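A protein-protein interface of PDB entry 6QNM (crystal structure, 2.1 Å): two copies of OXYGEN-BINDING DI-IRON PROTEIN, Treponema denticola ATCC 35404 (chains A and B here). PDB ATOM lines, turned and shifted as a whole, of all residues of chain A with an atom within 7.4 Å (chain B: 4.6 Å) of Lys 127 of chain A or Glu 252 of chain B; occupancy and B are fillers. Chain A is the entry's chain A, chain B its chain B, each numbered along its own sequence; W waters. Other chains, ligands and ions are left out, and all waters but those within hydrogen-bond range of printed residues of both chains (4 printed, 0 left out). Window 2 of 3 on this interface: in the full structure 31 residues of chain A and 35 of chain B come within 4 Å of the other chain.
Pro 125 of chain A touches none of the printed residues of chain B.
Lys 127 of chain A touches just these residues of chain B: Glu 252, Asn 253 and Phe 255.
Met 129 of chain A touches none of the printed residues of chain B.
Printed residues of chain B within 4 Å of Pro 143 of chain A: Leu 254 (3.2 Å) and Phe 255 (3.6 Å).
Printed residues of chain B within 4 Å of Lys 208 of chain A: Phe 255 (3.5 Å).
Of chain A, only Lys 127 comes within 4 Å of Glu 252 of chain B.
The nearest residue of chain B that does not touch Lys 127 of chain A is Leu 254 of chain B (4.5 Å).
The nearest residue of chain A that does not touch Glu 252 of chain B is Lys 208 of chain A (6.3 Å).
The nearest printed residue of chain B that does not touch Lys 208 of chain A is Ile 251 of chain B (4.2 Å).
Water W3 lies within hydrogen-bond range of OD1 of Asp 249 of chain B (2.7 Å) and NZ of Lys 204 of chain A (2.8 Å).
Water W2 lies within hydrogen-bond range of the side-chain amino group (NZ) of Lys 127 of chain A, the side-chain amide oxygen (OD1) of Asn 253 of chain B and the backbone carbonyl oxygen (O) of Glu 252 of chain B.
Water W1 lies within hydrogen-bond range of the backbone carbonyl oxygen of Leu 254 of chain B (3.0 Å), the backbone NH of His 145 of chain A (3.0 Å) and the backbone carbonyl oxygen of Pro 143 of chain A (3.4 Å).
Water W4 lies within hydrogen-bond range of the side-chain carboxylate of Asp 249 of chain B (3.1 Å) and the side-chain amino group of Lys 204 of chain A (3.4 Å).
NZ of Lys 127 of chain A is in hydrogen-bond range of O of Glu 252 of chain B (3.3 Å).
Printed residues of chain A that touch a printed residue of chain B: Asp 126, Lys 127, Pro 143, His 145, Lys 208 and Tyr 212.
Hydrophobic or aromatic side chains of chain A within 4 Å of the printed part of chain B: Pro 143, His 145 and Tyr 212.
Along chain A the printed residues that touch a printed residue of chain B span positions 126 to 212.
Hydrophobic or aromatic side chains of chain B that line the printed part of chain A: Phe 255.
Among the printed residues, no Asp or Glu carboxylate lies within 4 Å of a Lys or Arg side-chain nitrogen of the other chain.
No position is printed for both chains.
The backbone carbonyl oxygen of Asp 126 of chain A sits at hydrogen-bond distance from a ring nitrogen (NE2) of His 145 of chain A (2.8 Å).
Among the printed residues, merely in contact across the chains: Pro 143 of chain A with Leu 254 of chain B, Lys 127 of chain A with Phe 255 of chain B, Lys 208 of chain A with Phe 255 of chain B, His 145 of chain A with Leu 254 of chain B, Pro 143 of chain A with Phe 255 of chain B, Lys 127 of chain A with Asn 253 of chain B, Tyr 212 of chain A with Phe 255 of chain B, Asp 126 of chain A with Asn 253 of chain B and Asp 126 of chain A with Leu 254 of chain B.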
ATOM      1  N   ILE A 124     -18.521  13.129 -14.656  1.00  0.00           N
ATOM      2  CA  ILE A 124     -17.471  12.918 -15.648  1.00  0.00           C
ATOM      3  C   ILE A 124     -18.006  13.385 -17.000  1.00  0.00           C
ATOM      4  O   ILE A 124     -19.029  12.854 -17.460  1.00  0.00           O
ATOM      5  CB  ILE A 124     -17.035  11.451 -15.705  1.00  0.00           C
ATOM      6  CG1 ILE A 124     -16.663  10.946 -14.309  1.00  0.00           C
ATOM      7  CG2 ILE A 124     -15.856  11.279 -16.654  1.00  0.00           C
ATOM      8  CD1 ILE A 124     -16.514   9.442 -14.238  1.00  0.00           C
ATOM      9  N   PRO A 125     -17.361  14.347 -17.661  1.00  0.00           N
ATOM     10  CA  PRO A 125     -17.823  14.760 -18.989  1.00  0.00           C
ATOM     11  C   PRO A 125     -17.549  13.676 -20.017  1.00  0.00           C
ATOM     12  O   PRO A 125     -16.700  12.802 -19.827  1.00  0.00           O
ATOM     13  CB  PRO A 125     -17.008  16.026 -19.278  1.00  0.00           C
ATOM     14  CG  PRO A 125     -15.743  15.826 -18.496  1.00  0.00           C
ATOM     15  CD  PRO A 125     -16.116  15.030 -17.265  1.00  0.00           C
ATOM     16  N   ASP A 126     -18.269  13.775 -21.139  1.00  0.00           N
ATOM     17  CA  ASP A 126     -18.346  12.675 -22.099  1.00  0.00           C
ATOM     18  C   ASP A 126     -16.974  12.252 -22.612  1.00  0.00           C
ATOM     19  O   ASP A 126     -16.728  11.060 -22.828  1.00  0.00           O
ATOM     20  CB  ASP A 126     -19.254  13.073 -23.264  1.00  0.00           C
ATOM     21  CG  ASP A 126     -20.729  12.914 -22.929  1.00  0.00           C
ATOM     22  OD1 ASP A 126     -21.042  12.181 -21.965  1.00  0.00           O
ATOM     23  OD2 ASP A 126     -21.571  13.524 -23.620  1.00  0.00           O
ATOM     24  N   LYS A 127     -16.066  13.203 -22.807  1.00  0.00           N
ATOM     25  CA  LYS A 127     -14.754  12.888 -23.358  1.00  0.00           C
ATOM     26  C   LYS A 127     -13.731  12.543 -22.282  1.00  0.00           C
ATOM     27  O   LYS A 127     -12.545  12.393 -22.594  1.00  0.00           O
ATOM     28  CB  LYS A 127     -14.256  14.049 -24.225  1.00  0.00           C
ATOM     29  CG  LYS A 127     -14.914  14.072 -25.597  1.00  0.00           C
ATOM     30  CD  LYS A 127     -14.458  15.237 -26.455  1.00  0.00           C
ATOM     31  CE  LYS A 127     -15.378  15.401 -27.657  1.00  0.00           C
ATOM     32  NZ  LYS A 127     -14.766  16.214 -28.745  1.00  0.00           N
ATOM     33  N   GLY A 128     -14.165  12.396 -21.036  1.00  0.00           N
ATOM     34  CA  GLY A 128     -13.277  11.980 -19.972  1.00  0.00           C
ATOM     35  C   GLY A 128     -12.656  13.149 -19.239  1.00  0.00           C
ATOM     36  O   GLY A 128     -12.891  14.324 -19.535  1.00  0.00           O
ATOM     37  N   MET A 129     -11.833  12.801 -18.255  1.00  0.00           N
ATOM     38  CA  MET A 129     -11.119  13.774 -17.439  1.00  0.00           C
ATOM     39  C   MET A 129     -10.037  13.034 -16.669  1.00  0.00           C
ATOM     40  O   MET A 129     -10.075  11.806 -16.538  1.00  0.00           O
ATOM     41  CB  MET A 129     -12.060  14.501 -16.471  1.00  0.00           C
ATOM     42  CG  MET A 129     -12.327  13.724 -15.186  1.00  0.00           C
ATOM     43  SD  MET A 129     -13.670  14.390 -14.185  1.00  0.00           S
ATOM     44  CE  MET A 129     -13.430  16.126 -14.466  1.00  0.00           C
ATOM     45  N   CYS A 141     -10.283   8.845 -16.895  1.00  0.00           N
ATOM     46  CA  CYS A 141     -11.570   8.215 -17.177  1.00  0.00           C
ATOM     47  C   CYS A 141     -11.678   8.032 -18.682  1.00  0.00           C
ATOM     48  O   CYS A 141     -11.621   9.014 -19.425  1.00  0.00           O
ATOM     49  CB  CYS A 141     -12.712   9.100 -16.671  1.00  0.00           C
ATOM     50  SG  CYS A 141     -12.594   9.564 -14.933  1.00  0.00           S
ATOM     51  N   ILE A 142     -11.814   6.792 -19.135  1.00  0.00           N
ATOM     52  CA  ILE A 142     -11.713   6.455 -20.555  1.00  0.00           C
ATOM     53  C   ILE A 142     -13.126   6.356 -21.116  1.00  0.00           C
ATOM     54  O   ILE A 142     -13.893   5.493 -20.669  1.00  0.00           O
ATOM     55  CB  ILE A 142     -10.943   5.143 -20.789  1.00  0.00           C
ATOM     56  CG1 ILE A 142      -9.544   5.217 -20.166  1.00  0.00           C
ATOM     57  CG2 ILE A 142     -10.883   4.813 -22.284  1.00  0.00           C
ATOM     58  CD1 ILE A 142      -8.738   6.431 -20.594  1.00  0.00           C
ATOM     59  N   PRO A 143     -13.510   7.199 -22.073  1.00  0.00           N
ATOM     60  CA  PRO A 143     -14.881   7.142 -22.601  1.00  0.00           C
ATOM     61  C   PRO A 143     -15.206   5.762 -23.158  1.00  0.00           C
ATOM     62  O   PRO A 143     -14.454   5.199 -23.957  1.00  0.00           O
ATOM     63  CB  PRO A 143     -14.880   8.215 -23.696  1.00  0.00           C
ATOM     64  CG  PRO A 143     -13.795   9.169 -23.288  1.00  0.00           C
ATOM     65  CD  PRO A 143     -12.736   8.317 -22.636  1.00  0.00           C
ATOM     66  N   HIS A 145     -18.760   4.862 -23.911  1.00  0.00           N
ATOM     67  CA  HIS A 145     -20.197   5.016 -24.066  1.00  0.00           C
ATOM     68  C   HIS A 145     -20.768   3.993 -25.038  1.00  0.00           C
ATOM     69  O   HIS A 145     -20.127   3.607 -26.021  1.00  0.00           O
ATOM     70  CB  HIS A 145     -20.506   6.436 -24.533  1.00  0.00           C
ATOM     71  CG  HIS A 145     -19.872   7.483 -23.677  1.00  0.00           C
ATOM     72  ND1 HIS A 145     -20.163   7.615 -22.336  1.00  0.00           N
ATOM     73  CD2 HIS A 145     -18.954   8.439 -23.959  1.00  0.00           C
ATOM     74  CE1 HIS A 145     -19.461   8.613 -21.832  1.00  0.00           C
ATOM     75  NE2 HIS A 145     -18.722   9.132 -22.796  1.00  0.00           N
ATOM     76  N   PHE A 153     -17.705   4.736 -18.547  1.00  0.00           N
ATOM     77  CA  PHE A 153     -16.273   4.998 -18.535  1.00  0.00           C
ATOM     78  C   PHE A 153     -15.503   3.805 -17.991  1.00  0.00           C
ATOM     79  O   PHE A 153     -15.993   3.058 -17.140  1.00  0.00           O
ATOM     80  CB  PHE A 153     -15.936   6.240 -17.696  1.00  0.00           C
ATOM     81  CG  PHE A 153     -16.419   7.520 -18.311  1.00  0.00           C
ATOM     82  CD1 PHE A 153     -15.657   8.171 -19.269  1.00  0.00           C
ATOM     83  CD2 PHE A 153     -17.643   8.056 -17.952  1.00  0.00           C
ATOM     84  CE1 PHE A 153     -16.106   9.345 -19.852  1.00  0.00           C
ATOM     85  CE2 PHE A 153     -18.098   9.230 -18.531  1.00  0.00           C
ATOM     86  CZ  PHE A 153     -17.329   9.873 -19.484  1.00  0.00           C
ATOM     87  N   LYS A 204     -19.417  -0.167 -34.959  1.00  0.00           N
ATOM     88  CA  LYS A 204     -18.970   1.216 -35.100  1.00  0.00           C
ATOM     89  C   LYS A 204     -18.370   1.747 -33.801  1.00  0.00           C
ATOM     90  O   LYS A 204     -17.300   2.367 -33.805  1.00  0.00           O
ATOM     91  CB  LYS A 204     -20.136   2.098 -35.556  1.00  0.00           C
ATOM     92  CG  LYS A 204     -19.794   3.585 -35.651  1.00  0.00           C
ATOM     93  CD  LYS A 204     -20.969   4.394 -36.190  1.00  0.00           C
ATOM     94  CE  LYS A 204     -20.646   5.883 -36.238  1.00  0.00           C
ATOM     95  NZ  LYS A 204     -21.780   6.680 -36.793  1.00  0.00           N
ATOM     96  N   LYS A 208     -14.092   1.968 -32.717  1.00  0.00           N
ATOM     97  CA  LYS A 208     -13.567   3.270 -32.321  1.00  0.00           C
ATOM     98  C   LYS A 208     -12.970   3.209 -30.920  1.00  0.00           C
ATOM     99  O   LYS A 208     -11.934   3.828 -30.651  1.00  0.00           O
ATOM    100  CB  LYS A 208     -14.671   4.323 -32.396  1.00  0.00           C
ATOM    101  CG  LYS A 208     -14.192   5.743 -32.149  1.00  0.00           C
ATOM    102  CD  LYS A 208     -13.297   6.227 -33.277  1.00  0.00           C
ATOM    103  CE  LYS A 208     -14.113   6.739 -34.452  1.00  0.00           C
ATOM    104  NZ  LYS A 208     -13.580   8.034 -34.977  1.00  0.00           N
ATOM    105  N   TYR A 212      -9.076   3.958 -29.774  1.00  0.00           N
ATOM    106  CA  TYR A 212      -8.737   4.838 -28.659  1.00  0.00           C
ATOM    107  C   TYR A 212      -7.912   4.096 -27.616  1.00  0.00           C
ATOM    108  O   TYR A 212      -6.890   4.604 -27.136  1.00  0.00           O
ATOM    109  CB  TYR A 212     -10.021   5.393 -28.039  1.00  0.00           C
ATOM    110  CG  TYR A 212      -9.852   6.469 -26.980  1.00  0.00           C
ATOM    111  CD1 TYR A 212      -9.534   6.140 -25.667  1.00  0.00           C
ATOM    112  CD2 TYR A 212     -10.054   7.809 -27.288  1.00  0.00           C
ATOM    113  CE1 TYR A 212      -9.400   7.118 -24.695  1.00  0.00           C
ATOM    114  CE2 TYR A 212      -9.924   8.796 -26.322  1.00  0.00           C
ATOM    115  CZ  TYR A 212      -9.596   8.445 -25.028  1.00  0.00           C
ATOM    116  OH  TYR A 212      -9.465   9.419 -24.064  1.00  0.00           O
ATOM    117  N   ASP B 249     -24.331   8.466 -33.738  1.00  0.00           N
ATOM    118  CA  ASP B 249     -24.306   9.345 -34.901  1.00  0.00           C
ATOM    119  C   ASP B 249     -23.417  10.555 -34.649  1.00  0.00           C
ATOM    120  O   ASP B 249     -22.880  11.139 -35.596  1.00  0.00           O
ATOM    121  CB  ASP B 249     -25.716   9.815 -35.263  1.00  0.00           C
ATOM    122  CG  ASP B 249     -26.638   8.684 -35.670  1.00  0.00           C
ATOM    123  OD1 ASP B 249     -26.157   7.605 -36.080  1.00  0.00           O
ATOM    124  OD2 ASP B 249     -27.866   8.887 -35.584  1.00  0.00           O
ATOM    125  N   TYR B 250     -23.257  10.947 -33.385  1.00  0.00           N
ATOM    126  CA  TYR B 250     -22.346  12.018 -33.003  1.00  0.00           C
ATOM    127  C   TYR B 250     -21.103  11.430 -32.351  1.00  0.00           C
ATOM    128  O   TYR B 250     -20.689  11.884 -31.279  1.00  0.00           O
ATOM    129  CB  TYR B 250     -23.018  13.000 -32.041  1.00  0.00           C
ATOM    130  CG  TYR B 250     -24.151  13.798 -32.639  1.00  0.00           C
ATOM    131  CD1 TYR B 250     -23.902  14.915 -33.428  1.00  0.00           C
ATOM    132  CD2 TYR B 250     -25.471  13.445 -32.400  1.00  0.00           C
ATOM    133  CE1 TYR B 250     -24.940  15.649 -33.971  1.00  0.00           C
ATOM    134  CE2 TYR B 250     -26.512  14.171 -32.934  1.00  0.00           C
ATOM    135  CZ  TYR B 250     -26.245  15.273 -33.718  1.00  0.00           C
ATOM    136  OH  TYR B 250     -27.292  15.994 -34.250  1.00  0.00           O
ATOM    137  N   ILE B 251     -20.508  10.419 -32.991  1.00  0.00           N
ATOM    138  CA  ILE B 251     -19.360   9.722 -32.417  1.00  0.00           C
ATOM    139  C   ILE B 251     -18.208  10.668 -32.112  1.00  0.00           C
ATOM    140  O   ILE B 251     -17.398  10.390 -31.220  1.00  0.00           O
ATOM    141  CB  ILE B 251     -18.912   8.583 -33.358  1.00  0.00           C
ATOM    142  CG1 ILE B 251     -17.863   7.702 -32.684  1.00  0.00           C
ATOM    143  CG2 ILE B 251     -18.375   9.126 -34.667  1.00  0.00           C
ATOM    144  CD1 ILE B 251     -18.430   6.477 -32.064  1.00  0.00           C
ATOM    145  N   GLU B 252     -18.131  11.804 -32.813  1.00  0.00           N
ATOM    146  CA  GLU B 252     -17.075  12.778 -32.564  1.00  0.00           C
ATOM    147  C   GLU B 252     -17.161  13.387 -31.170  1.00  0.00           C
ATOM    148  O   GLU B 252     -16.145  13.858 -30.649  1.00  0.00           O
ATOM    149  CB  GLU B 252     -17.132  13.882 -33.621  1.00  0.00           C
ATOM    150  CG  GLU B 252     -18.349  14.794 -33.508  1.00  0.00           C
ATOM    151  CD  GLU B 252     -19.508  14.343 -34.383  1.00  0.00           C
ATOM    152  OE1 GLU B 252     -19.551  13.150 -34.750  1.00  0.00           O
ATOM    153  OE2 GLU B 252     -20.375  15.184 -34.703  1.00  0.00           O
ATOM    154  N   ASN B 253     -18.344  13.399 -30.560  1.00  0.00           N
ATOM    155  CA  ASN B 253     -18.518  13.938 -29.219  1.00  0.00           C
ATOM    156  C   ASN B 253     -18.268  12.907 -28.125  1.00  0.00           C
ATOM    157  O   ASN B 253     -18.305  13.261 -26.944  1.00  0.00           O
ATOM    158  CB  ASN B 253     -19.929  14.515 -29.050  1.00  0.00           C
ATOM    159  CG  ASN B 253     -20.251  15.607 -30.059  1.00  0.00           C
ATOM    160  OD1 ASN B 253     -19.358  16.208 -30.658  1.00  0.00           O
ATOM    161  ND2 ASN B 253     -21.539  15.872 -30.245  1.00  0.00           N
ATOM    162  N   LEU B 254     -18.025  11.648 -28.480  1.00  0.00           N
ATOM    163  CA  LEU B 254     -17.942  10.573 -27.498  1.00  0.00           C
ATOM    164  C   LEU B 254     -16.515  10.163 -27.162  1.00  0.00           C
ATOM    165  O   LEU B 254     -16.324   9.286 -26.312  1.00  0.00           O
ATOM    166  CB  LEU B 254     -18.724   9.350 -27.992  1.00  0.00           C
ATOM    167  CG  LEU B 254     -20.212   9.578 -28.275  1.00  0.00           C
ATOM    168  CD1 LEU B 254     -20.862   8.301 -28.798  1.00  0.00           C
ATOM    169  CD2 LEU B 254     -20.934  10.080 -27.032  1.00  0.00           C
ATOM    170  N   PHE B 255     -15.515  10.747 -27.813  1.00  0.00           N
ATOM    171  CA  PHE B 255     -14.122  10.435 -27.512  1.00  0.00           C
ATOM    172  C   PHE B 255     -13.271  11.698 -27.505  1.00  0.00           C
ATOM    173  O   PHE B 255     -13.528  12.623 -28.276  1.00  0.00           O
ATOM    174  CB  PHE B 255     -13.563   9.433 -28.522  1.00  0.00           C
ATOM    175  CG  PHE B 255     -14.202   8.076 -28.450  1.00  0.00           C
ATOM    176  CD1 PHE B 255     -15.308   7.773 -29.233  1.00  0.00           C
ATOM    177  CD2 PHE B 255     -13.694   7.099 -27.606  1.00  0.00           C
ATOM    178  CE1 PHE B 255     -15.902   6.520 -29.171  1.00  0.00           C
ATOM    179  CE2 PHE B 255     -14.281   5.846 -27.539  1.00  0.00           C
ATOM    180  CZ  PHE B 255     -15.385   5.555 -28.325  1.00  0.00           C
HETATM  181  O   HOH W   1     -17.063   6.451 -25.823  1.00  0.00           O
HETATM  182  O   HOH W   2     -16.686  17.194 -30.401  1.00  0.00           O
HETATM  183  O   HOH W   3     -24.134   5.951 -35.516  1.00  0.00           O
HETATM  184  O   HOH W   4     -24.397   8.065 -38.554  1.00  0.00           O
